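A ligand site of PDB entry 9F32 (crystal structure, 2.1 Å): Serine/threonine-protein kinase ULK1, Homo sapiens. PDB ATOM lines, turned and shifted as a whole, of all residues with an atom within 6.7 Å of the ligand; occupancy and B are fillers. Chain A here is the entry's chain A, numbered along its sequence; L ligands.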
ATOM      1  N   ILE A  24      21.810  19.094   5.403  1.00  0.00           N
ATOM      2  CA  ILE A  24      20.317  19.022   5.424  1.00  0.00           C
ATOM      3  C   ILE A  24      19.937  17.758   4.668  1.00  0.00           C
ATOM      4  O   ILE A  24      19.005  17.121   5.102  1.00  0.00           O
ATOM      5  CB  ILE A  24      19.663  20.234   4.730  1.00  0.00           C
ATOM      6  CG1 ILE A  24      19.601  21.466   5.629  1.00  0.00           C
ATOM      7  CG2 ILE A  24      18.289  19.869   4.181  1.00  0.00           C
ATOM      8  CD1 ILE A  24      18.857  22.625   5.012  1.00  0.00           C
ATOM      9  N   GLY A  25      20.605  17.502   3.545  1.00  0.00           N
ATOM     10  CA  GLY A  25      20.250  16.385   2.668  1.00  0.00           C
ATOM     11  C   GLY A  25      21.169  16.247   1.484  1.00  0.00           C
ATOM     12  O   GLY A  25      22.111  17.074   1.327  1.00  0.00           O
ATOM     13  N   HIS A  26      20.905  15.190   0.702  1.00  0.00           N
ATOM     14  CA  HIS A  26      21.619  14.826  -0.547  1.00  0.00           C
ATOM     15  C   HIS A  26      20.593  14.662  -1.655  1.00  0.00           C
ATOM     16  O   HIS A  26      19.470  14.195  -1.344  1.00  0.00           O
ATOM     17  CB  HIS A  26      22.428  13.548  -0.347  1.00  0.00           C
ATOM     18  CG  HIS A  26      23.172  13.511   0.933  1.00  0.00           C
ATOM     19  ND1 HIS A  26      24.536  13.781   1.020  1.00  0.00           N
ATOM     20  CD2 HIS A  26      22.760  13.198   2.181  1.00  0.00           C
ATOM     21  CE1 HIS A  26      24.924  13.653   2.271  1.00  0.00           C
ATOM     22  NE2 HIS A  26      23.854  13.276   2.999  1.00  0.00           N
ATOM     23  N   GLY A  27      20.959  15.061  -2.869  1.00  0.00           N
ATOM     24  CA  GLY A  27      20.213  14.813  -4.113  1.00  0.00           C
ATOM     25  C   GLY A  27      21.099  14.130  -5.126  1.00  0.00           C
ATOM     26  O   GLY A  27      22.121  13.544  -4.721  1.00  0.00           O
ATOM     27  N   ALA A  28      20.741  14.248  -6.404  1.00  0.00           N
ATOM     28  CA  ALA A  28      21.567  13.825  -7.563  1.00  0.00           C
ATOM     29  C   ALA A  28      22.865  14.640  -7.579  1.00  0.00           C
ATOM     30  O   ALA A  28      22.815  15.841  -7.905  1.00  0.00           O
ATOM     31  CB  ALA A  28      20.768  14.012  -8.833  1.00  0.00           C
ATOM     32  N   VAL A  32      22.864  19.566   0.370  1.00  0.00           N
ATOM     33  CA  VAL A  32      22.135  20.760   0.873  1.00  0.00           C
ATOM     34  C   VAL A  32      22.608  21.010   2.290  1.00  0.00           C
ATOM     35  O   VAL A  32      22.505  20.081   3.107  1.00  0.00           O
ATOM     36  CB  VAL A  32      20.610  20.603   0.797  1.00  0.00           C
ATOM     37  CG1 VAL A  32      19.951  21.937   1.113  1.00  0.00           C
ATOM     38  CG2 VAL A  32      20.165  20.092  -0.570  1.00  0.00           C
ATOM     39  N   VAL A  45      18.699  29.873   5.476  1.00  0.00           N
ATOM     40  CA  VAL A  45      18.608  29.445   4.052  1.00  0.00           C
ATOM     41  C   VAL A  45      19.091  27.992   3.971  1.00  0.00           C
ATOM     42  O   VAL A  45      19.719  27.498   4.950  1.00  0.00           O
ATOM     43  CB  VAL A  45      19.411  30.387   3.145  1.00  0.00           C
ATOM     44  CG1 VAL A  45      18.931  31.823   3.270  1.00  0.00           C
ATOM     45  CG2 VAL A  45      20.890  30.274   3.409  1.00  0.00           C
ATOM     46  N   ALA A  46      18.701  27.330   2.890  1.00  0.00           N
ATOM     47  CA  ALA A  46      19.278  26.052   2.406  1.00  0.00           C
ATOM     48  C   ALA A  46      20.231  26.384   1.256  1.00  0.00           C
ATOM     49  O   ALA A  46      19.840  27.093   0.328  1.00  0.00           O
ATOM     50  CB  ALA A  46      18.190  25.099   1.970  1.00  0.00           C
ATOM     51  N   LYS A  48      22.305  24.694  -1.727  1.00  0.00           N
ATOM     52  CA  LYS A  48      22.440  23.465  -2.518  1.00  0.00           C
ATOM     53  C   LYS A  48      23.741  23.593  -3.284  1.00  0.00           C
ATOM     54  O   LYS A  48      23.917  24.565  -4.002  1.00  0.00           O
ATOM     55  CB  LYS A  48      21.213  23.276  -3.420  1.00  0.00           C
ATOM     56  CG  LYS A  48      21.063  21.878  -4.012  1.00  0.00           C
ATOM     57  CD  LYS A  48      19.889  21.654  -4.944  1.00  0.00           C
ATOM     58  CE  LYS A  48      19.459  20.195  -4.967  1.00  0.00           C
ATOM     59  NZ  LYS A  48      18.889  19.783  -6.271  1.00  0.00           N
ATOM     60  N   VAL A  78       9.545  26.950  -3.231  1.00  0.00           N
ATOM     61  CA  VAL A  78      10.785  27.334  -2.507  1.00  0.00           C
ATOM     62  C   VAL A  78      11.438  28.458  -3.316  1.00  0.00           C
ATOM     63  O   VAL A  78      11.783  28.194  -4.493  1.00  0.00           O
ATOM     64  CB  VAL A  78      11.723  26.123  -2.349  1.00  0.00           C
ATOM     65  CG1 VAL A  78      13.063  26.558  -1.805  1.00  0.00           C
ATOM     66  CG2 VAL A  78      11.082  25.054  -1.473  1.00  0.00           C
ATOM     67  N   MET A  94      18.533  29.018  -1.187  1.00  0.00           N
ATOM     68  CA  MET A  94      17.071  28.803  -1.279  1.00  0.00           C
ATOM     69  C   MET A  94      16.450  29.182   0.052  1.00  0.00           C
ATOM     70  O   MET A  94      17.125  29.102   1.052  1.00  0.00           O
ATOM     71  CB  MET A  94      16.768  27.336  -1.586  1.00  0.00           C
ATOM     72  CG  MET A  94      17.266  26.881  -2.955  1.00  0.00           C
ATOM     73  SD  MET A  94      17.293  25.076  -3.025  1.00  0.00           S
ATOM     74  CE  MET A  94      15.887  24.710  -4.086  1.00  0.00           C
ATOM     75  N   GLU A  95      15.173  29.528   0.032  1.00  0.00           N
ATOM     76  CA  GLU A  95      14.286  29.648   1.219  1.00  0.00           C
ATOM     77  C   GLU A  95      14.439  28.392   2.083  1.00  0.00           C
ATOM     78  O   GLU A  95      14.356  27.262   1.552  1.00  0.00           O
ATOM     79  CB  GLU A  95      12.867  29.834   0.680  1.00  0.00           C
ATOM     80  CG  GLU A  95      11.786  29.844   1.728  1.00  0.00           C
ATOM     81  CD  GLU A  95      10.392  29.975   1.122  1.00  0.00           C
ATOM     82  OE1 GLU A  95      10.260  30.038  -0.139  1.00  0.00           O
ATOM     83  OE2 GLU A  95       9.441  30.040   1.899  1.00  0.00           O
ATOM     84  N   TYR A  96      14.671  28.575   3.370  1.00  0.00           N
ATOM     85  CA  TYR A  96      14.712  27.483   4.363  1.00  0.00           C
ATOM     86  C   TYR A  96      13.281  27.094   4.792  1.00  0.00           C
ATOM     87  O   TYR A  96      12.536  27.995   5.227  1.00  0.00           O
ATOM     88  CB  TYR A  96      15.515  27.901   5.586  1.00  0.00           C
ATOM     89  CG  TYR A  96      15.538  26.772   6.577  1.00  0.00           C
ATOM     90  CD1 TYR A  96      16.229  25.599   6.290  1.00  0.00           C
ATOM     91  CD2 TYR A  96      14.813  26.840   7.750  1.00  0.00           C
ATOM     92  CE1 TYR A  96      16.221  24.539   7.167  1.00  0.00           C
ATOM     93  CE2 TYR A  96      14.792  25.784   8.630  1.00  0.00           C
ATOM     94  CZ  TYR A  96      15.502  24.626   8.338  1.00  0.00           C
ATOM     95  OH  TYR A  96      15.528  23.579   9.223  1.00  0.00           O
ATOM     96  N   CYS A  97      12.922  25.804   4.661  1.00  0.00           N
ATOM     97  CA  CYS A  97      11.634  25.215   5.102  1.00  0.00           C
ATOM     98  C   CYS A  97      11.864  24.338   6.336  1.00  0.00           C
ATOM     99  O   CYS A  97      12.663  23.425   6.224  1.00  0.00           O
ATOM    100  CB  CYS A  97      11.021  24.426   3.955  1.00  0.00           C
ATOM    101  SG  CYS A  97      10.740  25.416   2.473  1.00  0.00           S
ATOM    102  N   ASN A  98      11.166  24.610   7.435  1.00  0.00           N
ATOM    103  CA  ASN A  98      11.446  24.129   8.819  1.00  0.00           C
ATOM    104  C   ASN A  98      10.686  22.830   9.161  1.00  0.00           C
ATOM    105  O   ASN A  98      10.895  22.306  10.251  1.00  0.00           O
ATOM    106  CB  ASN A  98      11.083  25.210   9.842  1.00  0.00           C
ATOM    107  CG  ASN A  98       9.598  25.524   9.914  1.00  0.00           C
ATOM    108  OD1 ASN A  98       8.819  25.116   9.060  1.00  0.00           O
ATOM    109  ND2 ASN A  98       9.191  26.283  10.919  1.00  0.00           N
ATOM    110  N   ASP A 101       9.716  17.138   5.062  1.00  0.00           N
ATOM    111  CA  ASP A 101       9.118  16.864   3.727  1.00  0.00           C
ATOM    112  C   ASP A 101       7.870  16.009   3.872  1.00  0.00           C
ATOM    113  O   ASP A 101       7.604  15.541   4.963  1.00  0.00           O
ATOM    114  CB  ASP A 101      10.128  16.249   2.766  1.00  0.00           C
ATOM    115  CG  ASP A 101      10.650  14.901   3.212  1.00  0.00           C
ATOM    116  OD1 ASP A 101       9.955  14.232   4.020  1.00  0.00           O
ATOM    117  OD2 ASP A 101      11.693  14.520   2.716  1.00  0.00           O
ATOM    118  N   ASP A 140      10.391  15.416 -11.699  1.00  0.00           N
ATOM    119  CA  ASP A 140      10.791  14.505 -10.590  1.00  0.00           C
ATOM    120  C   ASP A 140      10.066  14.934  -9.328  1.00  0.00           C
ATOM    121  O   ASP A 140      10.660  14.893  -8.257  1.00  0.00           O
ATOM    122  CB  ASP A 140      12.304  14.398 -10.390  1.00  0.00           C
ATOM    123  CG  ASP A 140      12.688  13.109  -9.683  1.00  0.00           C
ATOM    124  OD1 ASP A 140      11.974  12.088  -9.876  1.00  0.00           O
ATOM    125  OD2 ASP A 140      13.684  13.134  -8.915  1.00  0.00           O
ATOM    126  N   LYS A 142       8.057  14.352  -6.133  1.00  0.00           N
ATOM    127  CA  LYS A 142       7.936  13.222  -5.201  1.00  0.00           C
ATOM    128  C   LYS A 142       7.856  13.756  -3.772  1.00  0.00           C
ATOM    129  O   LYS A 142       8.103  14.931  -3.512  1.00  0.00           O
ATOM    130  CB  LYS A 142       9.131  12.276  -5.373  1.00  0.00           C
ATOM    131  CG  LYS A 142      10.490  12.927  -5.218  1.00  0.00           C
ATOM    132  CD  LYS A 142      11.516  12.309  -6.168  1.00  0.00           C
ATOM    133  CE  LYS A 142      12.925  12.563  -5.714  1.00  0.00           C
ATOM    134  NZ  LYS A 142      13.005  12.471  -4.247  1.00  0.00           N
ATOM    135  N   GLN A 144       9.633  13.620  -1.199  1.00  0.00           N
ATOM    136  CA  GLN A 144      10.900  14.180  -0.626  1.00  0.00           C
ATOM    137  C   GLN A 144      11.214  15.564  -1.225  1.00  0.00           C
ATOM    138  O   GLN A 144      12.058  16.269  -0.666  1.00  0.00           O
ATOM    139  CB  GLN A 144      12.030  13.181  -0.876  1.00  0.00           C
ATOM    140  CG  GLN A 144      11.696  11.766  -0.430  1.00  0.00           C
ATOM    141  CD  GLN A 144      11.262  10.870  -1.576  1.00  0.00           C
ATOM    142  OE1 GLN A 144      10.128  10.905  -2.083  1.00  0.00           O
ATOM    143  NE2 GLN A 144      12.205  10.053  -2.024  1.00  0.00           N
ATOM    144  N   ASN A 145      10.573  15.968  -2.313  1.00  0.00           N
ATOM    145  CA  ASN A 145      10.741  17.302  -2.947  1.00  0.00           C
ATOM    146  C   ASN A 145       9.586  18.237  -2.574  1.00  0.00           C
ATOM    147  O   ASN A 145       9.557  19.381  -3.117  1.00  0.00           O
ATOM    148  CB  ASN A 145      10.684  17.186  -4.480  1.00  0.00           C
ATOM    149  CG  ASN A 145      11.997  16.809  -5.093  1.00  0.00           C
ATOM    150  OD1 ASN A 145      13.053  16.991  -4.475  1.00  0.00           O
ATOM    151  ND2 ASN A 145      11.945  16.308  -6.311  1.00  0.00           N
ATOM    152  N   LEU A 147       8.097  20.131   0.388  1.00  0.00           N
ATOM    153  CA  LEU A 147       8.554  20.503   1.737  1.00  0.00           C
ATOM    154  C   LEU A 147       7.411  21.182   2.482  1.00  0.00           C
ATOM    155  O   LEU A 147       6.536  21.784   1.876  1.00  0.00           O
ATOM    156  CB  LEU A 147       9.807  21.385   1.662  1.00  0.00           C
ATOM    157  CG  LEU A 147      10.902  20.876   0.730  1.00  0.00           C
ATOM    158  CD1 LEU A 147      12.153  21.732   0.808  1.00  0.00           C
ATOM    159  CD2 LEU A 147      11.240  19.431   0.992  1.00  0.00           C
ATOM    160  N   ALA A 166      10.152  22.056  -4.190  1.00  0.00           N
ATOM    161  CA  ALA A 166      11.615  22.241  -4.298  1.00  0.00           C
ATOM    162  C   ALA A 166      12.118  21.497  -5.538  1.00  0.00           C
ATOM    163  O   ALA A 166      11.400  20.540  -6.022  1.00  0.00           O
ATOM    164  CB  ALA A 166      12.207  21.692  -3.021  1.00  0.00           C
ATOM    165  N   ASP A 167      13.322  21.857  -5.988  1.00  0.00           N
ATOM    166  CA  ASP A 167      14.094  21.176  -7.065  1.00  0.00           C
ATOM    167  C   ASP A 167      13.479  21.556  -8.424  1.00  0.00           C
ATOM    168  O   ASP A 167      13.887  20.984  -9.416  1.00  0.00           O
ATOM    169  CB  ASP A 167      14.182  19.651  -6.874  1.00  0.00           C
ATOM    170  CG  ASP A 167      15.459  19.096  -6.245  1.00  0.00           C
ATOM    171  OD1 ASP A 167      16.413  19.888  -5.992  1.00  0.00           O
ATOM    172  OD2 ASP A 167      15.519  17.842  -5.998  1.00  0.00           O
ATOM    173  N   CYS A 184      16.230  10.986  -2.789  1.00  0.00           N
ATOM    174  CA  CYS A 184      15.850  10.845  -4.223  1.00  0.00           C
ATOM    175  C   CYS A 184      15.883   9.327  -4.525  1.00  0.00           C
ATOM    176  O   CYS A 184      15.495   8.550  -3.619  1.00  0.00           O
ATOM    177  CB  CYS A 184      16.727  11.728  -5.127  1.00  0.00           C
ATOM    178  SG  CYS A 184      16.682  13.564  -4.990  1.00  0.00           S
ATOM    179  N   GLY A 185      16.243   8.890  -5.732  1.00  0.00           N
ATOM    180  CA  GLY A 185      16.375   7.449  -6.051  1.00  0.00           C
ATOM    181  C   GLY A 185      15.060   6.707  -6.288  1.00  0.00           C
ATOM    182  O   GLY A 185      15.113   5.699  -7.032  1.00  0.00           O
HETATM  183  C1  LIG L   1      15.516  14.689  -4.292  1.00  0.00           C
HETATM  184  C2  LIG L   1      14.937  14.717  -2.951  1.00  0.00           C
HETATM  185  C3  LIG L   1      15.763  14.707  -1.709  1.00  0.00           C
HETATM  186  O1  LIG L   1      15.680  13.841  -0.835  1.00  0.00           O
HETATM  187  N1  LIG L   1      16.619  15.724  -1.629  1.00  0.00           N
HETATM  188  C4  LIG L   1      16.378  17.029  -1.175  1.00  0.00           C
HETATM  189  C5  LIG L   1      15.488  17.880  -1.821  1.00  0.00           C
HETATM  190  C6  LIG L   1      15.307  19.164  -1.333  1.00  0.00           C
HETATM  191  C7  LIG L   1      16.005  19.627  -0.229  1.00  0.00           C
HETATM  192  C8  LIG L   1      15.765  20.984   0.324  1.00  0.00           C
HETATM  193  C9  LIG L   1      15.614  22.093  -0.562  1.00  0.00           C
HETATM  194  C10 LIG L   1      15.335  23.357  -0.099  1.00  0.00           C
HETATM  195  C11 LIG L   1      15.195  23.529   1.289  1.00  0.00           C
HETATM  196  N2  LIG L   1      14.864  24.616   2.024  1.00  0.00           N
HETATM  197  N3  LIG L   1      14.797  24.318   3.349  1.00  0.00           N
HETATM  198  C12 LIG L   1      15.066  23.030   3.451  1.00  0.00           C
HETATM  199  C13 LIG L   1      15.311  22.450   2.180  1.00  0.00           C
HETATM  200  C14 LIG L   1      15.604  21.169   1.693  1.00  0.00           C
HETATM  201  C15 LIG L   1      16.893  18.754   0.397  1.00  0.00           C
HETATM  202  C16 LIG L   1      17.100  17.476  -0.074  1.00  0.00           C
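A carbon (C1) of the ligand is covalently linked to the side-chain sulfur (SG) of Cys 184 (1.8 Å).
N of Cys 97 is in hydrogen-bond range of N3 of the ligand.
The backbone carbonyl oxygen (O) of Glu 95 sits at hydrogen-bond distance from a nitrogen (N2) of the ligand.
O of His 26 is in hydrogen-bond range of N1 of the ligand (3.2 Å).
NZ of Lys 142 lies close to NE2 of Gln 144, at 3.4 Å.
The side-chain amide oxygen of Asn 145 lies close to the side-chain carboxylate of Asp 167 (3.0 Å).
The backbone NH (N) of Ala 166 sits at hydrogen-bond distance from the backbone carbonyl oxygen (O) of Asn 145, at 2.9 Å.
The side-chain amide nitrogen of Asn 145 is in hydrogen-bond range of the backbone carbonyl oxygen of Asp 140, at 2.7 Å.
The backbone NH of Met 94 is in hydrogen-bond range of the backbone carbonyl oxygen of Ala 46 (2.8 Å).
The side-chain amino group (NZ) of Lys 48 lies within salt-bridge range of the side-chain carboxylate (OD1) of Asp 167 (2.5 Å).
N of Ile 24 sits at hydrogen-bond distance from O of Val 32, at 2.6 Å.
The backbone NH of Val 32 lies within hydrogen-bond range of the backbone carbonyl oxygen of Gly 25 (2.8 Å).
Merely in contact with the ligand: Lys 142, Asn 145, Tyr 96, Ala 46, Leu 147, Asp 167, Val 32, Gln 144, Ile 24 and Met 94.
Hydrophobic or aromatic side chains within 4 Å of the ligand: Ile 24, Val 32, Ala 46, Met 94, Tyr 96 and Leu 147.
Within 4 Å of the ligand: Ile 24, His 26, Val 32, Ala 46, Met 94, Glu 95, Tyr 96, Cys 97, Lys 142, Gln 144, Asn 145, Leu 147, Asp 167 and Cys 184.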
